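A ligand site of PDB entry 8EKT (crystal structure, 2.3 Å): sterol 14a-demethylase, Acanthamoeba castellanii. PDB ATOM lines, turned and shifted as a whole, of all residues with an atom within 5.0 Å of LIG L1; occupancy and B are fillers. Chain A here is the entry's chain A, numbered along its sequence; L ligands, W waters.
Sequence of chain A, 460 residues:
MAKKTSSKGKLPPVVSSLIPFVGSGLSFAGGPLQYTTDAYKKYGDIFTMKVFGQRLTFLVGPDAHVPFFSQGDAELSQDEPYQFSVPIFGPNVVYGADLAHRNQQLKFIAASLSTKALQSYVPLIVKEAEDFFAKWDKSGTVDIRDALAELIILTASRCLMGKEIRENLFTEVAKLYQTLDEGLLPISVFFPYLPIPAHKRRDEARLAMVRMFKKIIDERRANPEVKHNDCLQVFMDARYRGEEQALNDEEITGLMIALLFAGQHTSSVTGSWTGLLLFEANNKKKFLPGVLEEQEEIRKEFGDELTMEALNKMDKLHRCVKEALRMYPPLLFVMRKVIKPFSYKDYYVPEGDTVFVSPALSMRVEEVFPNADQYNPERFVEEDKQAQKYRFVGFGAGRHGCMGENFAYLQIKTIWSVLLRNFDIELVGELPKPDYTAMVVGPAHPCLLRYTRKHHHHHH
O2 of LIG L1 lies within hydrogen-bond range of OH of Tyr 82. A nitrogen (N4) of LG2 L2 sits close to the side-chain hydroxyl of Thr 266 (3.4 Å). A ring nitrogen (ND1) of His 400 sits at hydrogen-bond distance from an oxygen (O3) of LIG L1 (2.8 Å). The side-chain sulfur of Cys 402 binds an iron atom (FE1) of LIG L1 (2.2 Å). O1 of LIG L1 is in salt-bridge range of NH2 of Arg 336 (2.8 Å). O4 of LIG L1 sits at hydrogen-bond distance from OH of Tyr 95.
N5 of LG2 L2 binds FE1 of LIG L1 (2.2 Å).
OG1 of Thr 270 lies within hydrogen-bond range of O of Thr 266 (3.4 Å). The side-chain amide oxygen (OE1) of Gln 78 sits close to a ring nitrogen (NE2) of His 400 (3.4 Å). The side-chain sulfur of Cys 402 lies close to the backbone NH of Glu 405. The side-chain hydroxyl (OG1) of Thr 266 sits at hydrogen-bond distance from the backbone carbonyl oxygen (O) of Ala 262 (2.7 Å). OH of Tyr 82 sits at hydrogen-bond distance from NH1 of Arg 336. The side-chain sulfur (SG) of Cys 402 sits close to the backbone NH (N) of Gly 404 (3.2 Å). The backbone carbonyl oxygen (O) of Phe 395 lies within hydrogen-bond range of the backbone NH (N) of Cys 402 (3.0 Å).
Gln 78 touches LIG L1 (NE2 to O2, 3.6 Å). Leu 106 touches LIG L1 (CD1 to O3, 3.95 Å). Ile 109 touches LIG L1. CD1 of Leu 113 touches C25 of LIG L1, at 3.8 Å. Leu 259 touches LIG L1. Ala 262 touches LIG L1. Thr 266 touches LIG L1. Ser 267 touches LIG L1 (OG to C24, 3.5 Å). CD1 of Leu 325 touches C17 of LIG L1 (3.7 Å). Pro 330 touches LIG L1. Leu 331 touches LIG L1. Val 334 touches LIG L1 (CG1 to C12, 3.6 Å). Gly 394 touches LIG L1. Phe 395 touches LIG L1 (C to C9, 3.5 Å). Gly 396 touches LIG L1 (N to C9, 3.3 Å). Gly 401 touches LIG L1. Met 403 touches LIG L1. Gly 404 touches LIG L1 (CA to C22, 3.5 Å). CD2 of Phe 407 touches C24 of LIG L1 (3.7 Å). Ala 408 touches LIG L1. Hydrophobic or aromatic side chains that line LIG L1: Tyr 82, Leu 106, Ile 109, Leu 113, Leu 259, Ala 262, Leu 325, Pro 330, Leu 331, Val 334, Phe 395, His 400, Met 403, Phe 407 and Ala 408.
Water W2 lies within hydrogen-bond range of O1 of LIG L1 (2.6 Å) and O of His 400 (3.4 Å). Water W1 lies within hydrogen-bond range of the side-chain hydroxyl of Tyr 95 (2.7 Å), an oxygen (O2) of LG2 L2 (2.7 Å) and an oxygen (O2) of LIG L1 (3.0 Å).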
ATOM      1  N   GLN A  78     -12.133  -7.115   1.034  1.00  0.00           N
ATOM      2  CA  GLN A  78     -11.938  -6.478   2.334  1.00  0.00           C
ATOM      3  C   GLN A  78     -10.583  -6.869   2.933  1.00  0.00           C
ATOM      4  O   GLN A  78     -10.176  -6.300   3.944  1.00  0.00           O
ATOM      5  CB  GLN A  78     -13.046  -6.887   3.313  1.00  0.00           C
ATOM      6  CG  GLN A  78     -14.423  -6.380   2.928  1.00  0.00           C
ATOM      7  CD  GLN A  78     -15.498  -6.874   3.862  1.00  0.00           C
ATOM      8  OE1 GLN A  78     -15.768  -8.075   3.959  1.00  0.00           O
ATOM      9  NE2 GLN A  78     -16.128  -5.955   4.575  1.00  0.00           N
ATOM     10  N   TYR A  82      -8.220  -4.381   5.785  1.00  0.00           N
ATOM     11  CA  TYR A  82      -8.631  -4.703   7.151  1.00  0.00           C
ATOM     12  C   TYR A  82      -7.680  -5.739   7.770  1.00  0.00           C
ATOM     13  O   TYR A  82      -8.016  -6.351   8.783  1.00  0.00           O
ATOM     14  CB  TYR A  82     -10.073  -5.215   7.152  1.00  0.00           C
ATOM     15  CG  TYR A  82     -11.121  -4.214   6.754  1.00  0.00           C
ATOM     16  CD1 TYR A  82     -10.870  -2.858   6.723  1.00  0.00           C
ATOM     17  CD2 TYR A  82     -12.409  -4.633   6.450  1.00  0.00           C
ATOM     18  CE1 TYR A  82     -11.864  -1.937   6.384  1.00  0.00           C
ATOM     19  CE2 TYR A  82     -13.400  -3.747   6.104  1.00  0.00           C
ATOM     20  CZ  TYR A  82     -13.125  -2.399   6.061  1.00  0.00           C
ATOM     21  OH  TYR A  82     -14.148  -1.541   5.717  1.00  0.00           O
ATOM     22  N   TYR A  95     -11.532 -11.469   8.793  1.00  0.00           N
ATOM     23  CA  TYR A  95     -10.765 -11.026   7.630  1.00  0.00           C
ATOM     24  C   TYR A  95      -9.454 -11.809   7.570  1.00  0.00           C
ATOM     25  O   TYR A  95      -8.712 -11.679   6.596  1.00  0.00           O
ATOM     26  CB  TYR A  95     -10.556  -9.512   7.634  1.00  0.00           C
ATOM     27  CG  TYR A  95     -11.842  -8.724   7.711  1.00  0.00           C
ATOM     28  CD1 TYR A  95     -12.847  -8.916   6.782  1.00  0.00           C
ATOM     29  CD2 TYR A  95     -12.115  -7.910   8.798  1.00  0.00           C
ATOM     30  CE1 TYR A  95     -14.076  -8.298   6.912  1.00  0.00           C
ATOM     31  CE2 TYR A  95     -13.349  -7.284   8.946  1.00  0.00           C
ATOM     32  CZ  TYR A  95     -14.339  -7.483   8.002  1.00  0.00           C
ATOM     33  OH  TYR A  95     -15.583  -6.881   8.112  1.00  0.00           O
ATOM     34  N   LEU A 106     -19.817 -15.216   9.178  1.00  0.00           N
ATOM     35  CA  LEU A 106     -20.685 -14.063   9.152  1.00  0.00           C
ATOM     36  C   LEU A 106     -22.141 -14.493   9.340  1.00  0.00           C
ATOM     37  O   LEU A 106     -22.945 -13.740   9.901  1.00  0.00           O
ATOM     38  CB  LEU A 106     -20.495 -13.315   7.827  1.00  0.00           C
ATOM     39  CG  LEU A 106     -19.187 -12.527   7.717  1.00  0.00           C
ATOM     40  CD1 LEU A 106     -18.991 -11.986   6.298  1.00  0.00           C
ATOM     41  CD2 LEU A 106     -19.165 -11.388   8.726  1.00  0.00           C
ATOM     42  N   ILE A 109     -22.558 -15.107  12.988  1.00  0.00           N
ATOM     43  CA  ILE A 109     -22.692 -13.832  13.682  1.00  0.00           C
ATOM     44  C   ILE A 109     -24.109 -13.309  13.503  1.00  0.00           C
ATOM     45  O   ILE A 109     -24.753 -12.906  14.468  1.00  0.00           O
ATOM     46  CB  ILE A 109     -21.619 -12.822  13.208  1.00  0.00           C
ATOM     47  CG1 ILE A 109     -20.229 -13.251  13.689  1.00  0.00           C
ATOM     48  CG2 ILE A 109     -21.949 -11.412  13.687  1.00  0.00           C
ATOM     49  CD1 ILE A 109     -19.094 -12.506  13.040  1.00  0.00           C
ATOM     50  N   LEU A 113     -27.146 -12.496  16.353  1.00  0.00           N
ATOM     51  CA  LEU A 113     -27.693 -11.149  16.512  1.00  0.00           C
ATOM     52  C   LEU A 113     -29.040 -11.011  15.783  1.00  0.00           C
ATOM     53  O   LEU A 113     -29.473  -9.901  15.490  1.00  0.00           O
ATOM     54  CB  LEU A 113     -26.718 -10.119  15.945  1.00  0.00           C
ATOM     55  CG  LEU A 113     -25.324 -10.092  16.554  1.00  0.00           C
ATOM     56  CD1 LEU A 113     -24.404  -9.211  15.718  1.00  0.00           C
ATOM     57  CD2 LEU A 113     -25.362  -9.631  18.002  1.00  0.00           C
ATOM     58  N   LEU A 259     -16.854  -9.102  18.182  1.00  0.00           N
ATOM     59  CA  LEU A 259     -18.134  -8.476  18.518  1.00  0.00           C
ATOM     60  C   LEU A 259     -17.975  -7.545  19.732  1.00  0.00           C
ATOM     61  O   LEU A 259     -18.692  -6.555  19.863  1.00  0.00           O
ATOM     62  CB  LEU A 259     -19.154  -9.569  18.817  1.00  0.00           C
ATOM     63  CG  LEU A 259     -19.562 -10.460  17.635  1.00  0.00           C
ATOM     64  CD1 LEU A 259     -20.853 -11.201  17.933  1.00  0.00           C
ATOM     65  CD2 LEU A 259     -19.731  -9.653  16.357  1.00  0.00           C
ATOM     66  N   ALA A 262     -16.464  -4.456  18.259  1.00  0.00           N
ATOM     67  CA  ALA A 262     -17.482  -3.683  17.548  1.00  0.00           C
ATOM     68  C   ALA A 262     -18.187  -2.738  18.508  1.00  0.00           C
ATOM     69  O   ALA A 262     -18.320  -1.540  18.225  1.00  0.00           O
ATOM     70  CB  ALA A 262     -18.473  -4.616  16.881  1.00  0.00           C
ATOM     71  N   GLY A 263     -18.706  -3.286  19.609  1.00  0.00           N
ATOM     72  CA  GLY A 263     -19.478  -2.512  20.552  1.00  0.00           C
ATOM     73  C   GLY A 263     -18.681  -1.353  21.135  1.00  0.00           C
ATOM     74  O   GLY A 263     -19.197  -0.257  21.294  1.00  0.00           O
ATOM     75  N   THR A 266     -18.011   1.388  18.251  1.00  0.00           N
ATOM     76  CA  THR A 266     -19.105   2.055  17.550  1.00  0.00           C
ATOM     77  C   THR A 266     -20.202   2.450  18.528  1.00  0.00           C
ATOM     78  O   THR A 266     -20.563   3.623  18.624  1.00  0.00           O
ATOM     79  CB  THR A 266     -19.629   1.181  16.405  1.00  0.00           C
ATOM     80  OG1 THR A 266     -20.132  -0.058  16.930  1.00  0.00           O
ATOM     81  CG2 THR A 266     -18.565   0.884  15.365  1.00  0.00           C
ATOM     82  N   SER A 267     -20.838   1.456  19.148  1.00  0.00           N
ATOM     83  CA  SER A 267     -22.028   1.676  19.946  1.00  0.00           C
ATOM     84  C   SER A 267     -21.726   2.664  21.068  1.00  0.00           C
ATOM     85  O   SER A 267     -22.512   3.569  21.325  1.00  0.00           O
ATOM     86  CB  SER A 267     -22.548   0.372  20.493  1.00  0.00           C
ATOM     87  OG  SER A 267     -23.138  -0.420  19.463  1.00  0.00           O
ATOM     88  N   THR A 270     -21.409   6.353  19.574  1.00  0.00           N
ATOM     89  CA  THR A 270     -22.687   6.869  19.103  1.00  0.00           C
ATOM     90  C   THR A 270     -23.648   7.026  20.287  1.00  0.00           C
ATOM     91  O   THR A 270     -24.518   7.890  20.267  1.00  0.00           O
ATOM     92  CB  THR A 270     -23.264   5.981  17.993  1.00  0.00           C
ATOM     93  OG1 THR A 270     -22.316   6.030  16.923  1.00  0.00           O
ATOM     94  CG2 THR A 270     -24.618   6.422  17.497  1.00  0.00           C
ATOM     95  N   LEU A 325     -25.584   9.645  14.744  1.00  0.00           N
ATOM     96  CA  LEU A 325     -24.785   8.783  13.890  1.00  0.00           C
ATOM     97  C   LEU A 325     -24.482   9.488  12.571  1.00  0.00           C
ATOM     98  O   LEU A 325     -23.365   9.446  12.082  1.00  0.00           O
ATOM     99  CB  LEU A 325     -25.531   7.461  13.692  1.00  0.00           C
ATOM    100  CG  LEU A 325     -24.931   6.501  12.661  1.00  0.00           C
ATOM    101  CD1 LEU A 325     -23.450   6.257  12.947  1.00  0.00           C
ATOM    102  CD2 LEU A 325     -25.680   5.186  12.650  1.00  0.00           C
ATOM    103  N   PRO A 330     -18.824   6.779  13.850  1.00  0.00           N
ATOM    104  CA  PRO A 330     -17.631   6.311  14.568  1.00  0.00           C
ATOM    105  C   PRO A 330     -16.534   5.718  13.693  1.00  0.00           C
ATOM    106  O   PRO A 330     -15.371   5.663  14.097  1.00  0.00           O
ATOM    107  CB  PRO A 330     -18.150   5.227  15.529  1.00  0.00           C
ATOM    108  CG  PRO A 330     -19.496   4.815  14.968  1.00  0.00           C
ATOM    109  CD  PRO A 330     -20.040   6.022  14.211  1.00  0.00           C
ATOM    110  N   LEU A 331     -16.918   5.167  12.536  1.00  0.00           N
ATOM    111  CA  LEU A 331     -15.945   4.658  11.589  1.00  0.00           C
ATOM    112  C   LEU A 331     -15.656   5.743  10.559  1.00  0.00           C
ATOM    113  O   LEU A 331     -16.560   6.126   9.818  1.00  0.00           O
ATOM    114  CB  LEU A 331     -16.499   3.416  10.889  1.00  0.00           C
ATOM    115  CG  LEU A 331     -16.709   2.177  11.759  1.00  0.00           C
ATOM    116  CD1 LEU A 331     -17.322   1.061  10.945  1.00  0.00           C
ATOM    117  CD2 LEU A 331     -15.403   1.725  12.381  1.00  0.00           C
ATOM    118  N   VAL A 334     -14.829   3.210   5.463  1.00  0.00           N
ATOM    119  CA  VAL A 334     -14.858   1.820   5.070  1.00  0.00           C
ATOM    120  C   VAL A 334     -14.115   1.698   3.740  1.00  0.00           C
ATOM    121  O   VAL A 334     -14.003   2.684   3.022  1.00  0.00           O
ATOM    122  CB  VAL A 334     -16.310   1.314   5.000  1.00  0.00           C
ATOM    123  CG1 VAL A 334     -16.934   1.228   6.384  1.00  0.00           C
ATOM    124  CG2 VAL A 334     -17.179   2.174   4.107  1.00  0.00           C
ATOM    125  N   ARG A 336     -12.251  -0.933   0.441  1.00  0.00           N
ATOM    126  CA  ARG A 336     -12.114  -2.151  -0.331  1.00  0.00           C
ATOM    127  C   ARG A 336     -10.889  -2.032  -1.246  1.00  0.00           C
ATOM    128  O   ARG A 336     -10.536  -0.937  -1.655  1.00  0.00           O
ATOM    129  CB  ARG A 336     -13.360  -2.418  -1.190  1.00  0.00           C
ATOM    130  CG  ARG A 336     -14.683  -2.404  -0.437  1.00  0.00           C
ATOM    131  CD  ARG A 336     -15.018  -3.692   0.293  1.00  0.00           C
ATOM    132  NE  ARG A 336     -16.308  -3.667   0.972  1.00  0.00           N
ATOM    133  CZ  ARG A 336     -16.523  -3.125   2.178  1.00  0.00           C
ATOM    134  NH1 ARG A 336     -15.503  -2.799   2.956  1.00  0.00           N
ATOM    135  NH2 ARG A 336     -17.770  -2.992   2.613  1.00  0.00           N
ATOM    136  N   VAL A 393     -25.289   6.228   5.298  1.00  0.00           N
ATOM    137  CA  VAL A 393     -24.351   5.117   5.227  1.00  0.00           C
ATOM    138  C   VAL A 393     -23.600   4.981   6.551  1.00  0.00           C
ATOM    139  O   VAL A 393     -22.504   4.408   6.587  1.00  0.00           O
ATOM    140  CB  VAL A 393     -23.373   5.297   4.056  1.00  0.00           C
ATOM    141  CG1 VAL A 393     -24.100   5.202   2.722  1.00  0.00           C
ATOM    142  CG2 VAL A 393     -22.595   6.597   4.149  1.00  0.00           C
ATOM    143  N   GLY A 394     -24.247   5.344   7.666  1.00  0.00           N
ATOM    144  CA  GLY A 394     -23.659   5.178   8.975  1.00  0.00           C
ATOM    145  C   GLY A 394     -23.436   3.710   9.340  1.00  0.00           C
ATOM    146  O   GLY A 394     -22.496   3.383  10.070  1.00  0.00           O
ATOM    147  N   PHE A 395     -24.320   2.838   8.838  1.00  0.00           N
ATOM    148  CA  PHE A 395     -24.183   1.405   9.039  1.00  0.00           C
ATOM    149  C   PHE A 395     -23.727   0.701   7.760  1.00  0.00           C
ATOM    150  O   PHE A 395     -23.933  -0.503   7.608  1.00  0.00           O
ATOM    151  CB  PHE A 395     -25.500   0.781   9.494  1.00  0.00           C
ATOM    152  CG  PHE A 395     -25.943   1.185  10.867  1.00  0.00           C
ATOM    153  CD1 PHE A 395     -25.301   0.676  11.996  1.00  0.00           C
ATOM    154  CD2 PHE A 395     -26.978   2.091  11.049  1.00  0.00           C
ATOM    155  CE1 PHE A 395     -25.714   1.050  13.267  1.00  0.00           C
ATOM    156  CE2 PHE A 395     -27.361   2.473  12.325  1.00  0.00           C
ATOM    157  CZ  PHE A 395     -26.733   1.958  13.431  1.00  0.00           C
ATOM    158  N   GLY A 396     -23.055   1.455   6.879  1.00  0.00           N
ATOM    159  CA  GLY A 396     -22.691   0.888   5.594  1.00  0.00           C
ATOM    160  C   GLY A 396     -23.947   0.530   4.804  1.00  0.00           C
ATOM    161  O   GLY A 396     -25.006   1.092   5.064  1.00  0.00           O
ATOM    162  N   ARG A 399     -23.857  -5.816   0.655  1.00  0.00           N
ATOM    163  CA  ARG A 399     -23.505  -7.160   1.075  1.00  0.00           C
ATOM    164  C   ARG A 399     -22.917  -7.146   2.491  1.00  0.00           C
ATOM    165  O   ARG A 399     -23.123  -8.097   3.244  1.00  0.00           O
ATOM    166  CB  ARG A 399     -22.526  -7.746   0.039  1.00  0.00           C
ATOM    167  CG  ARG A 399     -21.856  -9.044   0.446  1.00  0.00           C
ATOM    168  CD  ARG A 399     -22.816 -10.226   0.440  1.00  0.00           C
ATOM    169  NE  ARG A 399     -22.411 -11.272   1.382  1.00  0.00           N
ATOM    170  CZ  ARG A 399     -21.222 -11.858   1.383  1.00  0.00           C
ATOM    171  NH1 ARG A 399     -20.406 -11.687   0.369  1.00  0.00           N
ATOM    172  NH2 ARG A 399     -20.872 -12.620   2.406  1.00  0.00           N
ATOM    173  N   HIS A 400     -22.119  -6.123   2.827  1.00  0.00           N
ATOM    174  CA  HIS A 400     -21.379  -6.133   4.084  1.00  0.00           C
ATOM    175  C   HIS A 400     -21.853  -5.012   5.008  1.00  0.00           C
ATOM    176  O   HIS A 400     -21.124  -4.563   5.884  1.00  0.00           O
ATOM    177  CB  HIS A 400     -19.871  -6.046   3.828  1.00  0.00           C
ATOM    178  CG  HIS A 400     -19.297  -7.261   3.196  1.00  0.00           C
ATOM    179  ND1 HIS A 400     -19.140  -8.473   3.851  1.00  0.00           N
ATOM    180  CD2 HIS A 400     -18.773  -7.447   1.972  1.00  0.00           C
ATOM    181  CE1 HIS A 400     -18.575  -9.345   3.043  1.00  0.00           C
ATOM    182  NE2 HIS A 400     -18.352  -8.741   1.887  1.00  0.00           N
ATOM    183  N   GLY A 401     -23.125  -4.662   4.899  1.00  0.00           N
ATOM    184  CA  GLY A 401     -23.696  -3.718   5.866  1.00  0.00           C
ATOM    185  C   GLY A 401     -23.685  -4.281   7.289  1.00  0.00           C
ATOM    186  O   GLY A 401     -23.555  -5.495   7.443  1.00  0.00           O
ATOM    187  N   CYS A 402     -23.867  -3.416   8.281  1.00  0.00           N
ATOM    188  CA  CYS A 402     -23.764  -3.815   9.709  1.00  0.00           C
ATOM    189  C   CYS A 402     -24.813  -4.868  10.106  1.00  0.00           C
ATOM    190  O   CYS A 402     -26.012  -4.601   9.996  1.00  0.00           O
ATOM    191  CB  CYS A 402     -23.846  -2.606  10.647  1.00  0.00           C
ATOM    192  SG  CYS A 402     -23.544  -2.964  12.387  1.00  0.00           S
ATOM    193  N   MET A 403     -24.303  -5.989  10.594  1.00  0.00           N
ATOM    194  CA  MET A 403     -25.179  -7.061  11.107  1.00  0.00           C
ATOM    195  C   MET A 403     -25.589  -6.711  12.545  1.00  0.00           C
ATOM    196  O   MET A 403     -26.491  -7.378  13.042  1.00  0.00           O
ATOM    197  CB  MET A 403     -24.404  -8.380  11.061  1.00  0.00           C
ATOM    198  CG  MET A 403     -24.556  -9.133   9.753  1.00  0.00           C
ATOM    199  SD  MET A 403     -23.631 -10.691   9.659  1.00  0.00           S
ATOM    200  CE  MET A 403     -22.054 -10.223  10.355  1.00  0.00           C
ATOM    201  N   GLY A 404     -24.983  -5.688  13.138  1.00  0.00           N
ATOM    202  CA  GLY A 404     -25.236  -5.326  14.540  1.00  0.00           C
ATOM    203  C   GLY A 404     -26.094  -4.099  14.689  1.00  0.00           C
ATOM    204  O   GLY A 404     -26.197  -3.596  15.798  1.00  0.00           O
ATOM    205  N   GLU A 405     -26.712  -3.659  13.583  1.00  0.00           N
ATOM    206  CA  GLU A 405     -27.482  -2.432  13.613  1.00  0.00           C
ATOM    207  C   GLU A 405     -28.575  -2.498  14.681  1.00  0.00           C
ATOM    208  O   GLU A 405     -28.747  -1.583  15.466  1.00  0.00           O
ATOM    209  CB  GLU A 405     -28.041  -2.176  12.208  1.00  0.00           C
ATOM    210  CG  GLU A 405     -29.052  -1.044  12.171  1.00  0.00           C
ATOM    211  CD  GLU A 405     -29.417  -0.547  10.781  1.00  0.00           C
ATOM    212  OE1 GLU A 405     -28.777  -1.011   9.795  1.00  0.00           O
ATOM    213  OE2 GLU A 405     -30.307   0.346  10.687  1.00  0.00           O
ATOM    214  N   PHE A 407     -29.088  -4.527  17.219  1.00  0.00           N
ATOM    215  CA  PHE A 407     -28.532  -4.644  18.566  1.00  0.00           C
ATOM    216  C   PHE A 407     -28.107  -3.258  19.068  1.00  0.00           C
ATOM    217  O   PHE A 407     -28.389  -2.902  20.217  1.00  0.00           O
ATOM    218  CB  PHE A 407     -27.391  -5.670  18.553  1.00  0.00           C
ATOM    219  CG  PHE A 407     -26.644  -5.804  19.853  1.00  0.00           C
ATOM    220  CD1 PHE A 407     -27.322  -5.797  21.071  1.00  0.00           C
ATOM    221  CD2 PHE A 407     -25.271  -5.996  19.872  1.00  0.00           C
ATOM    222  CE1 PHE A 407     -26.645  -5.954  22.258  1.00  0.00           C
ATOM    223  CE2 PHE A 407     -24.588  -6.106  21.075  1.00  0.00           C
ATOM    224  CZ  PHE A 407     -25.279  -6.065  22.263  1.00  0.00           C
ATOM    225  N   ALA A 408     -27.451  -2.484  18.207  1.00  0.00           N
ATOM    226  CA  ALA A 408     -26.919  -1.185  18.597  1.00  0.00           C
ATOM    227  C   ALA A 408     -28.063  -0.270  19.001  1.00  0.00           C
ATOM    228  O   ALA A 408     -27.984   0.398  20.030  1.00  0.00           O
ATOM    229  CB  ALA A 408     -26.114  -0.579  17.481  1.00  0.00           C
ATOM    230  N   ILE A 412     -28.735   1.273  22.710  1.00  0.00           N
ATOM    231  CA  ILE A 412     -28.538   2.696  22.926  1.00  0.00           C
ATOM    232  C   ILE A 412     -29.865   3.318  23.351  1.00  0.00           C
ATOM    233  O   ILE A 412     -29.896   4.176  24.224  1.00  0.00           O
ATOM    234  CB  ILE A 412     -27.971   3.395  21.667  1.00  0.00           C
ATOM    235  CG1 ILE A 412     -26.550   2.910  21.349  1.00  0.00           C
ATOM    236  CG2 ILE A 412     -28.007   4.898  21.826  1.00  0.00           C
ATOM    237  CD1 ILE A 412     -26.014   3.380  20.017  1.00  0.00           C
HETATM  238  C1  LIG L   1     -20.256  -3.773   9.711  1.00  0.00           C
HETATM  239  C2  LIG L   1     -21.267   0.551  11.597  1.00  0.00           C
HETATM  240  C3  LIG L   1     -22.579  -1.575  15.752  1.00  0.00           C
HETATM  241  C4  LIG L   1     -21.262  -5.846  13.959  1.00  0.00           C
HETATM  242  C5  LIG L   1     -20.450  -2.422   9.874  1.00  0.00           C
HETATM  243  C6  LIG L   1     -20.214  -1.468   8.882  1.00  0.00           C
HETATM  244  C7  LIG L   1     -20.496  -0.250   9.409  1.00  0.00           C
HETATM  245  C8  LIG L   1     -20.891  -0.442  10.726  1.00  0.00           C
HETATM  246  C9  LIG L   1     -20.386   1.071   8.699  1.00  0.00           C
HETATM  247  C10 LIG L   1     -19.742  -1.735   7.484  1.00  0.00           C
HETATM  248  C11 LIG L   1     -18.243  -2.040   7.497  1.00  0.00           C
HETATM  249  C12 LIG L   1     -17.731  -2.257   6.102  1.00  0.00           C
HETATM  250  O1  LIG L   1     -18.459  -2.037   5.121  1.00  0.00           O
HETATM  251  O2  LIG L   1     -16.570  -2.661   5.921  1.00  0.00           O
HETATM  252  C13 LIG L   1     -21.709   0.315  12.896  1.00  0.00           C
HETATM  253  C14 LIG L   1     -22.122   1.362  13.756  1.00  0.00           C
HETATM  254  C15 LIG L   1     -22.503   0.789  14.919  1.00  0.00           C
HETATM  255  C16 LIG L   1     -22.306  -0.664  14.743  1.00  0.00           C
HETATM  256  C17 LIG L   1     -22.130   2.820  13.404  1.00  0.00           C
HETATM  257  C18 LIG L   1     -22.993   1.462  16.134  1.00  0.00           C
HETATM  258  C19 LIG L   1     -23.970   2.362  16.090  1.00  0.00           C
HETATM  259  C20 LIG L   1     -22.328  -2.934  15.643  1.00  0.00           C
HETATM  260  C21 LIG L   1     -22.528  -3.875  16.653  1.00  0.00           C
HETATM  261  C22 LIG L   1     -22.148  -5.106  16.149  1.00  0.00           C
HETATM  262  C23 LIG L   1     -21.717  -4.881  14.818  1.00  0.00           C
HETATM  263  C24 LIG L   1     -23.059  -3.605  18.042  1.00  0.00           C
HETATM  264  C25 LIG L   1     -22.197  -6.390  16.862  1.00  0.00           C
HETATM  265  C26 LIG L   1     -21.574  -6.552  18.023  1.00  0.00           C
HETATM  266  C27 LIG L   1     -20.889  -5.575  12.648  1.00  0.00           C
HETATM  267  C28 LIG L   1     -20.432  -6.660  11.782  1.00  0.00           C
HETATM  268  C29 LIG L   1     -20.159  -6.106  10.595  1.00  0.00           C
HETATM  269  C30 LIG L   1     -20.441  -4.666  10.739  1.00  0.00           C
HETATM  270  C31 LIG L   1     -20.304  -8.117  12.148  1.00  0.00           C
HETATM  271  C32 LIG L   1     -19.616  -6.838   9.409  1.00  0.00           C
HETATM  272  C33 LIG L   1     -20.387  -6.655   8.116  1.00  0.00           C
HETATM  273  C34 LIG L   1     -19.718  -7.500   7.070  1.00  0.00           C
HETATM  274  O3  LIG L   1     -20.401  -8.292   6.382  1.00  0.00           O
HETATM  275  O4  LIG L   1     -18.486  -7.429   6.860  1.00  0.00           O
HETATM  276  N1  LIG L   1     -20.864  -1.777  11.011  1.00  0.00           N
HETATM  277  N2  LIG L   1     -21.834  -0.856  13.517  1.00  0.00           N
HETATM  278  N3  LIG L   1     -21.832  -3.553  14.543  1.00  0.00           N
HETATM  279  N4  LIG L   1     -20.877  -4.417  11.987  1.00  0.00           N
HETATM  280 FE1  LIG L   1     -21.361  -2.732  12.666  1.00  0.00          FE
HETATM  281  F1  LG2 L   2      -6.221   4.793   7.855  1.00  0.00           F
HETATM  282  C1  LG2 L   2      -7.138   5.212   8.721  1.00  0.00           C
HETATM  283  F2  LG2 L   2      -6.976   6.529   8.846  1.00  0.00           F
HETATM  284  F3  LG2 L   2      -6.834   4.673   9.896  1.00  0.00           F
HETATM  285  C2  LG2 L   2      -8.520   4.870   8.278  1.00  0.00           C
HETATM  286  O1  LG2 L   2      -9.382   4.975   9.412  1.00  0.00           O
HETATM  287  C3  LG2 L   2     -10.118   3.858   9.705  1.00  0.00           C
HETATM  288  C4  LG2 L   2      -9.501   2.645   9.523  1.00  0.00           C
HETATM  289  C5  LG2 L   2     -10.187   1.478   9.784  1.00  0.00           C
HETATM  290  C6  LG2 L   2     -11.440   3.903  10.142  1.00  0.00           C
HETATM  291  C7  LG2 L   2     -12.105   2.714  10.407  1.00  0.00           C
HETATM  292  C8  LG2 L   2     -11.496   1.489  10.217  1.00  0.00           C
HETATM  293  C9  LG2 L   2     -12.179   0.203  10.505  1.00  0.00           C
HETATM  294  C10 LG2 L   2     -12.352  -0.233  11.809  1.00  0.00           C
HETATM  295  N1  LG2 L   2     -12.919  -1.402  12.128  1.00  0.00           N
HETATM  296  C11 LG2 L   2     -12.598  -0.654   9.496  1.00  0.00           C
HETATM  297  C12 LG2 L   2     -13.185  -1.854   9.812  1.00  0.00           C
HETATM  298  C13 LG2 L   2     -13.355  -2.194  11.144  1.00  0.00           C
HETATM  299  C14 LG2 L   2     -13.947  -3.500  11.580  1.00  0.00           C
HETATM  300  F4  LG2 L   2     -13.342  -3.967  12.693  1.00  0.00           F
HETATM  301  F5  LG2 L   2     -13.753  -4.461  10.652  1.00  0.00           F
HETATM  302  C15 LG2 L   2     -15.464  -3.401  11.870  1.00  0.00           C
HETATM  303  C16 LG2 L   2     -15.715  -2.343  12.954  1.00  0.00           C
HETATM  304  N2  LG2 L   2     -17.116  -2.349  13.344  1.00  0.00           N
HETATM  305  N3  LG2 L   2     -17.508  -2.066  14.579  1.00  0.00           N
HETATM  306  N4  LG2 L   2     -18.789  -2.182  14.568  1.00  0.00           N
HETATM  307  N5  LG2 L   2     -19.231  -2.543  13.328  1.00  0.00           N
HETATM  308  C17 LG2 L   2     -18.182  -2.632  12.580  1.00  0.00           C
HETATM  309  O2  LG2 L   2     -16.108  -2.959  10.677  1.00  0.00           O
HETATM  310  C18 LG2 L   2     -15.966  -4.778  12.283  1.00  0.00           C
HETATM  311  C19 LG2 L   2     -15.950  -5.237  13.586  1.00  0.00           C
HETATM  312  F6  LG2 L   2     -15.467  -4.424  14.553  1.00  0.00           F
HETATM  313  C20 LG2 L   2     -16.385  -6.477  13.985  1.00  0.00           C
HETATM  314  C21 LG2 L   2     -16.874  -7.284  13.003  1.00  0.00           C
HETATM  315  F7  LG2 L   2     -17.317  -8.516  13.363  1.00  0.00           F
HETATM  316  C22 LG2 L   2     -16.929  -6.920  11.694  1.00  0.00           C
HETATM  317  C23 LG2 L   2     -16.477  -5.666  11.338  1.00  0.00           C
HETATM  318  O   HOH W   1     -15.723  -4.235   8.310  1.00  0.00           O
HETATM  319  O   HOH W   2     -20.811  -1.726   4.121  1.00  0.00           O
